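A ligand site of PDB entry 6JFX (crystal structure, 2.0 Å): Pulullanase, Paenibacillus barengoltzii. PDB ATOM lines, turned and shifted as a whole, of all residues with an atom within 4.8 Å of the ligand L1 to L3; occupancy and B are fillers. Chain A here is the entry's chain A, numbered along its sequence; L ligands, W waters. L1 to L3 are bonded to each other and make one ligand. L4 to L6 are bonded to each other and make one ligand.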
ATOM      1  N   THR A 314     -16.395  -4.629 -20.160  1.00  0.00           N
ATOM      2  CA  THR A 314     -17.578  -3.999 -19.575  1.00  0.00           C
ATOM      3  C   THR A 314     -17.241  -2.765 -18.748  1.00  0.00           C
ATOM      4  O   THR A 314     -18.142  -1.981 -18.434  1.00  0.00           O
ATOM      5  CB  THR A 314     -18.314  -4.995 -18.672  1.00  0.00           C
ATOM      6  OG1 THR A 314     -17.434  -5.391 -17.603  1.00  0.00           O
ATOM      7  CG2 THR A 314     -18.751  -6.251 -19.469  1.00  0.00           C
ATOM      8  N   PHE A 315     -15.964  -2.604 -18.373  1.00  0.00           N
ATOM      9  CA  PHE A 315     -15.522  -1.625 -17.369  1.00  0.00           C
ATOM     10  C   PHE A 315     -16.142  -1.872 -16.000  1.00  0.00           C
ATOM     11  O   PHE A 315     -16.210  -0.963 -15.174  1.00  0.00           O
ATOM     12  CB  PHE A 315     -15.771  -0.185 -17.830  1.00  0.00           C
ATOM     13  CG  PHE A 315     -15.229   0.111 -19.189  1.00  0.00           C
ATOM     14  CD1 PHE A 315     -13.860   0.172 -19.393  1.00  0.00           C
ATOM     15  CD2 PHE A 315     -16.069   0.296 -20.275  1.00  0.00           C
ATOM     16  CE1 PHE A 315     -13.337   0.427 -20.647  1.00  0.00           C
ATOM     17  CE2 PHE A 315     -15.562   0.555 -21.545  1.00  0.00           C
ATOM     18  CZ  PHE A 315     -14.197   0.618 -21.724  1.00  0.00           C
ATOM     19  N   LEU A 351     -25.362  -4.029 -22.366  1.00  0.00           N
ATOM     20  CA  LEU A 351     -24.089  -4.290 -23.073  1.00  0.00           C
ATOM     21  C   LEU A 351     -24.174  -5.554 -23.915  1.00  0.00           C
ATOM     22  O   LEU A 351     -23.390  -6.494 -23.754  1.00  0.00           O
ATOM     23  CB  LEU A 351     -22.922  -4.363 -22.096  1.00  0.00           C
ATOM     24  CG  LEU A 351     -22.658  -3.096 -21.282  1.00  0.00           C
ATOM     25  CD1 LEU A 351     -21.393  -3.272 -20.431  1.00  0.00           C
ATOM     26  CD2 LEU A 351     -22.564  -1.890 -22.227  1.00  0.00           C
ATOM     27  N   GLU A 379     -28.391  -3.039 -25.899  1.00  0.00           N
ATOM     28  CA  GLU A 379     -27.357  -2.045 -26.193  1.00  0.00           C
ATOM     29  C   GLU A 379     -26.354  -2.690 -27.131  1.00  0.00           C
ATOM     30  O   GLU A 379     -25.477  -3.424 -26.684  1.00  0.00           O
ATOM     31  CB  GLU A 379     -26.647  -1.595 -24.917  1.00  0.00           C
ATOM     32  CG  GLU A 379     -27.414  -0.691 -24.010  1.00  0.00           C
ATOM     33  CD  GLU A 379     -26.586  -0.340 -22.788  1.00  0.00           C
ATOM     34  OE1 GLU A 379     -26.222  -1.279 -22.037  1.00  0.00           O
ATOM     35  OE2 GLU A 379     -26.268   0.852 -22.613  1.00  0.00           O
ATOM     36  N   TRP A 381     -23.629  -1.724 -28.538  1.00  0.00           N
ATOM     37  CA  TRP A 381     -22.470  -0.861 -28.705  1.00  0.00           C
ATOM     38  C   TRP A 381     -21.250  -1.669 -29.121  1.00  0.00           C
ATOM     39  O   TRP A 381     -21.086  -2.833 -28.726  1.00  0.00           O
ATOM     40  CB  TRP A 381     -22.134  -0.081 -27.432  1.00  0.00           C
ATOM     41  CG  TRP A 381     -23.295   0.561 -26.692  1.00  0.00           C
ATOM     42  CD1 TRP A 381     -23.532   0.499 -25.341  1.00  0.00           C
ATOM     43  CD2 TRP A 381     -24.354   1.350 -27.250  1.00  0.00           C
ATOM     44  NE1 TRP A 381     -24.657   1.207 -25.027  1.00  0.00           N
ATOM     45  CE2 TRP A 381     -25.194   1.741 -26.177  1.00  0.00           C
ATOM     46  CE3 TRP A 381     -24.683   1.769 -28.549  1.00  0.00           C
ATOM     47  CZ2 TRP A 381     -26.336   2.530 -26.366  1.00  0.00           C
ATOM     48  CZ3 TRP A 381     -25.830   2.551 -28.741  1.00  0.00           C
ATOM     49  CH2 TRP A 381     -26.642   2.926 -27.643  1.00  0.00           C
ATOM     50  N   MET A 382     -20.396  -1.044 -29.930  1.00  0.00           N
ATOM     51  CA  MET A 382     -19.145  -1.638 -30.386  1.00  0.00           C
ATOM     52  C   MET A 382     -18.085  -1.414 -29.317  1.00  0.00           C
ATOM     53  O   MET A 382     -17.634  -0.283 -29.115  1.00  0.00           O
ATOM     54  CB  MET A 382     -18.717  -1.022 -31.714  1.00  0.00           C
ATOM     55  CG  MET A 382     -19.249  -1.733 -32.936  1.00  0.00           C
ATOM     56  SD  MET A 382     -21.032  -1.512 -33.149  1.00  0.00           S
ATOM     57  CE  MET A 382     -21.121   0.200 -33.709  1.00  0.00           C
ATOM     58  N   MET A 383     -17.667  -2.483 -28.638  1.00  0.00           N
ATOM     59  CA  MET A 383     -16.786  -2.349 -27.488  1.00  0.00           C
ATOM     60  C   MET A 383     -15.754  -3.472 -27.507  1.00  0.00           C
ATOM     61  O   MET A 383     -16.079  -4.616 -27.824  1.00  0.00           O
ATOM     62  CB  MET A 383     -17.599  -2.401 -26.174  1.00  0.00           C
ATOM     63  CG  MET A 383     -18.605  -1.256 -26.051  1.00  0.00           C
ATOM     64  SD  MET A 383     -19.716  -1.404 -24.641  1.00  0.00           S
ATOM     65  CE  MET A 383     -18.603  -1.090 -23.256  1.00  0.00           C
ATOM     66  N   ASP A 409     -28.302   5.152 -31.222  1.00  0.00           N
ATOM     67  CA  ASP A 409     -27.599   6.314 -30.656  1.00  0.00           C
ATOM     68  C   ASP A 409     -27.344   7.406 -31.699  1.00  0.00           C
ATOM     69  O   ASP A 409     -27.191   8.576 -31.348  1.00  0.00           O
ATOM     70  CB  ASP A 409     -26.280   5.880 -29.999  1.00  0.00           C
ATOM     71  CG  ASP A 409     -25.373   5.067 -30.942  1.00  0.00           C
ATOM     72  OD1 ASP A 409     -25.871   4.326 -31.809  1.00  0.00           O
ATOM     73  OD2 ASP A 409     -24.133   5.172 -30.790  1.00  0.00           O
ATOM     74  N   ARG A 412     -30.427   9.493 -31.492  1.00  0.00           N
ATOM     75  CA  ARG A 412     -30.431  10.165 -30.203  1.00  0.00           C
ATOM     76  C   ARG A 412     -29.565  11.418 -30.232  1.00  0.00           C
ATOM     77  O   ARG A 412     -30.016  12.513 -29.889  1.00  0.00           O
ATOM     78  CB  ARG A 412     -29.963   9.178 -29.140  1.00  0.00           C
ATOM     79  CG  ARG A 412     -29.617   9.803 -27.789  1.00  0.00           C
ATOM     80  CD  ARG A 412     -28.626   8.912 -27.049  1.00  0.00           C
ATOM     81  NE  ARG A 412     -27.259   9.114 -27.538  1.00  0.00           N
ATOM     82  CZ  ARG A 412     -26.263   8.231 -27.402  1.00  0.00           C
ATOM     83  NH1 ARG A 412     -26.480   7.067 -26.811  1.00  0.00           N
ATOM     84  NH2 ARG A 412     -25.050   8.518 -27.869  1.00  0.00           N
ATOM     85  N   ASP A 413     -28.312  11.282 -30.688  1.00  0.00           N
ATOM     86  CA  ASP A 413     -27.403  12.425 -30.718  1.00  0.00           C
ATOM     87  C   ASP A 413     -27.816  13.471 -31.759  1.00  0.00           C
ATOM     88  O   ASP A 413     -27.633  14.666 -31.543  1.00  0.00           O
ATOM     89  CB  ASP A 413     -25.972  11.949 -30.985  1.00  0.00           C
ATOM     90  CG  ASP A 413     -25.369  11.220 -29.788  1.00  0.00           C
ATOM     91  OD1 ASP A 413     -25.846  11.408 -28.655  1.00  0.00           O
ATOM     92  OD2 ASP A 413     -24.421  10.438 -30.006  1.00  0.00           O
ATOM     93  N   ILE A 419     -24.288  13.487 -26.333  1.00  0.00           N
ATOM     94  CA  ILE A 419     -24.481  13.238 -24.901  1.00  0.00           C
ATOM     95  C   ILE A 419     -23.182  13.303 -24.102  1.00  0.00           C
ATOM     96  O   ILE A 419     -23.231  13.393 -22.864  1.00  0.00           O
ATOM     97  CB  ILE A 419     -25.117  11.867 -24.609  1.00  0.00           C
ATOM     98  CG1 ILE A 419     -24.265  10.734 -25.195  1.00  0.00           C
ATOM     99  CG2 ILE A 419     -26.562  11.821 -25.135  1.00  0.00           C
ATOM    100  CD1 ILE A 419     -24.618   9.367 -24.619  1.00  0.00           C
ATOM    101  N   PHE A 420     -22.030  13.270 -24.758  1.00  0.00           N
ATOM    102  CA  PHE A 420     -20.762  13.331 -24.041  1.00  0.00           C
ATOM    103  C   PHE A 420     -20.112  14.705 -24.051  1.00  0.00           C
ATOM    104  O   PHE A 420     -19.211  14.942 -23.235  1.00  0.00           O
ATOM    105  CB  PHE A 420     -19.788  12.305 -24.625  1.00  0.00           C
ATOM    106  CG  PHE A 420     -20.266  10.885 -24.486  1.00  0.00           C
ATOM    107  CD1 PHE A 420     -20.661  10.401 -23.236  1.00  0.00           C
ATOM    108  CD2 PHE A 420     -20.369  10.056 -25.589  1.00  0.00           C
ATOM    109  CE1 PHE A 420     -21.118   9.091 -23.091  1.00  0.00           C
ATOM    110  CE2 PHE A 420     -20.837   8.745 -25.454  1.00  0.00           C
ATOM    111  CZ  PHE A 420     -21.210   8.270 -24.198  1.00  0.00           C
ATOM    112  N   ASP A 470     -29.365   6.391 -18.355  1.00  0.00           N
ATOM    113  CA  ASP A 470     -27.977   6.836 -18.529  1.00  0.00           C
ATOM    114  C   ASP A 470     -27.906   8.280 -19.024  1.00  0.00           C
ATOM    115  O   ASP A 470     -28.747   8.742 -19.789  1.00  0.00           O
ATOM    116  CB  ASP A 470     -27.251   5.945 -19.542  1.00  0.00           C
ATOM    117  CG  ASP A 470     -26.814   4.611 -18.951  1.00  0.00           C
ATOM    118  OD1 ASP A 470     -26.306   4.609 -17.816  1.00  0.00           O
ATOM    119  OD2 ASP A 470     -26.981   3.570 -19.625  1.00  0.00           O
ATOM    120  N   ASN A 471     -26.840   8.967 -18.600  1.00  0.00           N
ATOM    121  CA  ASN A 471     -26.480  10.300 -19.089  1.00  0.00           C
ATOM    122  C   ASN A 471     -27.540  11.314 -18.664  1.00  0.00           C
ATOM    123  O   ASN A 471     -28.486  10.961 -17.954  1.00  0.00           O
ATOM    124  CB  ASN A 471     -26.266  10.271 -20.609  1.00  0.00           C
ATOM    125  CG  ASN A 471     -25.339   9.143 -21.033  1.00  0.00           C
ATOM    126  OD1 ASN A 471     -24.147   9.133 -20.695  1.00  0.00           O
ATOM    127  ND2 ASN A 471     -25.873   8.177 -21.756  1.00  0.00           N
ATOM    128  N   GLU A 524     -25.124  13.582 -14.242  1.00  0.00           N
ATOM    129  CA  GLU A 524     -24.897  12.868 -15.491  1.00  0.00           C
ATOM    130  C   GLU A 524     -25.054  11.356 -15.344  1.00  0.00           C
ATOM    131  O   GLU A 524     -25.556  10.694 -16.268  1.00  0.00           O
ATOM    132  CB  GLU A 524     -23.487  13.172 -16.009  1.00  0.00           C
ATOM    133  CG  GLU A 524     -23.289  12.909 -17.489  1.00  0.00           C
ATOM    134  CD  GLU A 524     -22.921  11.478 -17.811  1.00  0.00           C
ATOM    135  OE1 GLU A 524     -23.087  11.078 -18.986  1.00  0.00           O
ATOM    136  OE2 GLU A 524     -22.463  10.754 -16.893  1.00  0.00           O
ATOM    137  N   ASN A 525     -24.600  10.779 -14.242  1.00  0.00           N
ATOM    138  CA  ASN A 525     -24.615   9.329 -14.074  1.00  0.00           C
ATOM    139  C   ASN A 525     -25.130   9.055 -12.664  1.00  0.00           C
ATOM    140  O   ASN A 525     -24.370   9.063 -11.705  1.00  0.00           O
ATOM    141  CB  ASN A 525     -23.203   8.777 -14.291  1.00  0.00           C
ATOM    142  CG  ASN A 525     -23.112   7.286 -14.081  1.00  0.00           C
ATOM    143  OD1 ASN A 525     -24.086   6.558 -14.246  1.00  0.00           O
ATOM    144  ND2 ASN A 525     -21.915   6.823 -13.709  1.00  0.00           N
HETATM  145  C1  LIG L   1     -21.424   4.747 -28.130  1.00  0.00           C
HETATM  146  C2  LIG L   1     -22.848   5.093 -27.681  1.00  0.00           C
HETATM  147  C3  LIG L   1     -22.867   5.469 -26.202  1.00  0.00           C
HETATM  148  C4  LIG L   1     -22.322   4.298 -25.406  1.00  0.00           C
HETATM  149  C5  LIG L   1     -20.918   3.974 -25.900  1.00  0.00           C
HETATM  150  C6  LIG L   1     -20.356   2.746 -25.184  1.00  0.00           C
HETATM  151  O1  LIG L   1     -20.555   5.890 -28.062  1.00  0.00           O
HETATM  152  O2  LIG L   1     -23.376   6.166 -28.475  1.00  0.00           O
HETATM  153  O3  LIG L   1     -24.192   5.751 -25.784  1.00  0.00           O
HETATM  154  O4  LIG L   1     -22.278   4.635 -24.018  1.00  0.00           O
HETATM  155  O5  LIG L   1     -20.927   3.696 -27.298  1.00  0.00           O
HETATM  156  O6  LIG L   1     -19.058   2.468 -25.733  1.00  0.00           O
HETATM  157  C1  LG2 L   2     -23.308   3.970 -23.261  1.00  0.00           C
HETATM  158  C2  LG2 L   2     -23.908   4.971 -22.284  1.00  0.00           C
HETATM  159  C3  LG2 L   2     -22.869   5.342 -21.236  1.00  0.00           C
HETATM  160  C4  LG2 L   2     -22.284   4.087 -20.593  1.00  0.00           C
HETATM  161  C5  LG2 L   2     -21.685   3.228 -21.707  1.00  0.00           C
HETATM  162  C6  LG2 L   2     -20.912   2.002 -21.203  1.00  0.00           C
HETATM  163  O1  LG2 L   2     -24.318   6.152 -22.998  1.00  0.00           O
HETATM  164  O2  LG2 L   2     -23.437   6.206 -20.242  1.00  0.00           O
HETATM  165  O3  LG2 L   2     -21.267   4.464 -19.659  1.00  0.00           O
HETATM  166  O4  LG2 L   2     -22.770   2.840 -22.540  1.00  0.00           O
HETATM  167  O5  LG2 L   2     -21.724   1.302 -20.263  1.00  0.00           O
HETATM  168  C1  LG3 L   3     -21.597   4.039 -18.323  1.00  0.00           C
HETATM  169  C2  LG3 L   3     -21.605   5.234 -17.363  1.00  0.00           C
HETATM  170  C3  LG3 L   3     -20.242   5.904 -17.412  1.00  0.00           C
HETATM  171  C4  LG3 L   3     -19.124   4.905 -17.150  1.00  0.00           C
HETATM  172  C5  LG3 L   3     -19.302   3.624 -17.982  1.00  0.00           C
HETATM  173  C6  LG3 L   3     -18.292   2.558 -17.562  1.00  0.00           C
HETATM  174  O1  LG3 L   3     -22.586   6.209 -17.730  1.00  0.00           O
HETATM  175  O2  LG3 L   3     -20.211   6.961 -16.443  1.00  0.00           O
HETATM  176  O3  LG3 L   3     -17.872   5.518 -17.489  1.00  0.00           O
HETATM  177  O4  LG3 L   3     -20.624   3.111 -17.842  1.00  0.00           O
HETATM  178  O5  LG3 L   3     -17.574   2.998 -16.399  1.00  0.00           O
HETATM  179  C1  LG4 L   4     -24.990  -0.159 -19.519  1.00  0.00           C
HETATM  180  C2  LG4 L   4     -26.004   0.390 -18.525  1.00  0.00           C
HETATM  181  C3  LG4 L   4     -25.261   1.361 -17.639  1.00  0.00           C
HETATM  182  C4  LG4 L   4     -24.334   0.521 -16.755  1.00  0.00           C
HETATM  183  C5  LG4 L   4     -23.396  -0.318 -17.629  1.00  0.00           C
HETATM  184  C6  LG4 L   4     -22.796  -1.450 -16.797  1.00  0.00           C
HETATM  185  O1  LG4 L   4     -24.405   0.887 -20.330  1.00  0.00           O
HETATM  186  O2  LG4 L   4     -27.136   0.973 -19.189  1.00  0.00           O
HETATM  187  O3  LG4 L   4     -26.179   2.146 -16.881  1.00  0.00           O
HETATM  188  O4  LG4 L   4     -23.542   1.378 -15.918  1.00  0.00           O
HETATM  189  O5  LG4 L   4     -24.030  -0.933 -18.782  1.00  0.00           O
HETATM  190  O6  LG4 L   4     -23.711  -2.559 -16.704  1.00  0.00           O
HETATM  191  C1  LG5 L   5     -24.112   1.700 -14.628  1.00  0.00           C
HETATM  192  C2  LG5 L   5     -23.429   2.985 -14.162  1.00  0.00           C
HETATM  193  C3  LG5 L   5     -21.937   2.722 -13.969  1.00  0.00           C
HETATM  194  C4  LG5 L   5     -21.762   1.596 -12.956  1.00  0.00           C
HETATM  195  C5  LG5 L   5     -22.518   0.371 -13.461  1.00  0.00           C
HETATM  196  C6  LG5 L   5     -22.334  -0.841 -12.533  1.00  0.00           C
HETATM  197  O1  LG5 L   5     -23.643   4.016 -15.143  1.00  0.00           O
HETATM  198  O2  LG5 L   5     -21.230   3.910 -13.563  1.00  0.00           O
HETATM  199  O3  LG5 L   5     -20.382   1.244 -12.811  1.00  0.00           O
HETATM  200  O4  LG5 L   5     -23.906   0.707 -13.614  1.00  0.00           O
HETATM  201  O5  LG5 L   5     -22.901  -0.547 -11.240  1.00  0.00           O
HETATM  202  C1  LG6 L   6     -19.920   1.571 -11.489  1.00  0.00           C
HETATM  203  C2  LG6 L   6     -18.611   2.346 -11.641  1.00  0.00           C
HETATM  204  C3  LG6 L   6     -17.552   1.433 -12.270  1.00  0.00           C
HETATM  205  C4  LG6 L   6     -17.381   0.222 -11.382  1.00  0.00           C
HETATM  206  C5  LG6 L   6     -18.715  -0.511 -11.212  1.00  0.00           C
HETATM  207  C6  LG6 L   6     -18.586  -1.707 -10.280  1.00  0.00           C
HETATM  208  O1  LG6 L   6     -18.810   3.495 -12.474  1.00  0.00           O
HETATM  209  O2  LG6 L   6     -16.305   2.117 -12.397  1.00  0.00           O
HETATM  210  O3  LG6 L   6     -16.386  -0.638 -11.974  1.00  0.00           O
HETATM  211  O4  LG6 L   6     -19.708   0.392 -10.685  1.00  0.00           O
HETATM  212  O5  LG6 L   6     -19.140  -1.362  -9.002  1.00  0.00           O
HETATM  213  O   HOH W   1     -19.971  -0.021 -18.453  1.00  0.00           O
HETATM  214  O   HOH W   2     -18.634   2.238 -28.642  1.00  0.00           O
HETATM  215  O   HOH W   3     -25.090   6.804 -16.817  1.00  0.00           O
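The guanidinium group (NE) of Arg 412 is in salt-bridge range of the side-chain carboxylate (OD1) of Asp 413 (2.9 Å).
The side-chain amide oxygen (OD1) of Asn 471 lies close to the side-chain carboxylate (OE1) of Glu 524 (2.8 Å).
The indole nitrogen (NE1) of Trp 381 sits at hydrogen-bond distance from the side-chain carboxylate (OE2) of Glu 379.
N of Ile 419 lies within hydrogen-bond range of OD1 of Asp 413, 3.5 Å away.
OE1 of Glu 379 sits at hydrogen-bond distance from N of Leu 351 (2.9 Å).
Residues that only touch the ligand L1 to L3: Phe 315, Leu 351, Trp 381, Met 383, Ile 419, Phe 420 and Asp 470.
Hydrophobic or aromatic side chains within 4 Å of the ligand L1 to L3: Phe 315, Leu 351, Trp 381, Met 383, Ile 419 and Phe 420.
11 residues have an atom within 4 Å of the ligand L1 to L3: Phe 315, Leu 351, Trp 381, Met 383, Asp 409, Arg 412, Ile 419, Phe 420, Asp 470, Asn 471 and Asn 525.
The nearest printed residue that does not touch the ligand L1 to L3 is Glu 379 (4.02 Å).
O1 of LG4 L4 is in hydrogen-bond range of O5 of LG2 L2, at 2.7 Å.
An oxygen (O2) of LIG L1 is in hydrogen-bond range of the side-chain carboxylate (OD2) of Asp 409 (2.6 Å).
The guanidinium group of Arg 412 sits at hydrogen-bond distance from an oxygen (O3) of LIG L1.
The side-chain amide nitrogen (ND2) of Asn 471 is in hydrogen-bond range of an oxygen (O1) of LG2 L2 (2.8 Å).
ND2 of Asn 525 sits at hydrogen-bond distance from O2 of LG3 L3 (3.2 Å).
An oxygen (O1) of LG5 L5 sits at hydrogen-bond distance from the side-chain amide oxygen (OD1) of Asn 525, 2.7 Å away.
The backbone carbonyl oxygen (O) of Phe 315 is in hydrogen-bond range of an oxygen (O3) of LG6 L6 (3.2 Å).
O3 of LG4 L4 is in hydrogen-bond range of OD1 of Asp 470, at 2.6 Å.
O1 of LG4 L4 sits at hydrogen-bond distance from OE2 of Glu 379 (2.9 Å).
Water W3 lies within hydrogen-bond range of OD1 of Asp 470 (2.7 Å), O1 of LG3 L3 (2.7 Å), OD1 of Asn 525 (2.8 Å) and N of Asn 471 (3.3 Å).
Water W1 lies within hydrogen-bond range of the backbone carbonyl oxygen (O) of Thr 314 (2.7 Å) and an oxygen (O5) of LG2 L2 (2.8 Å).
Water W2 bridges O of Met 382 and O6 of LIG L1.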
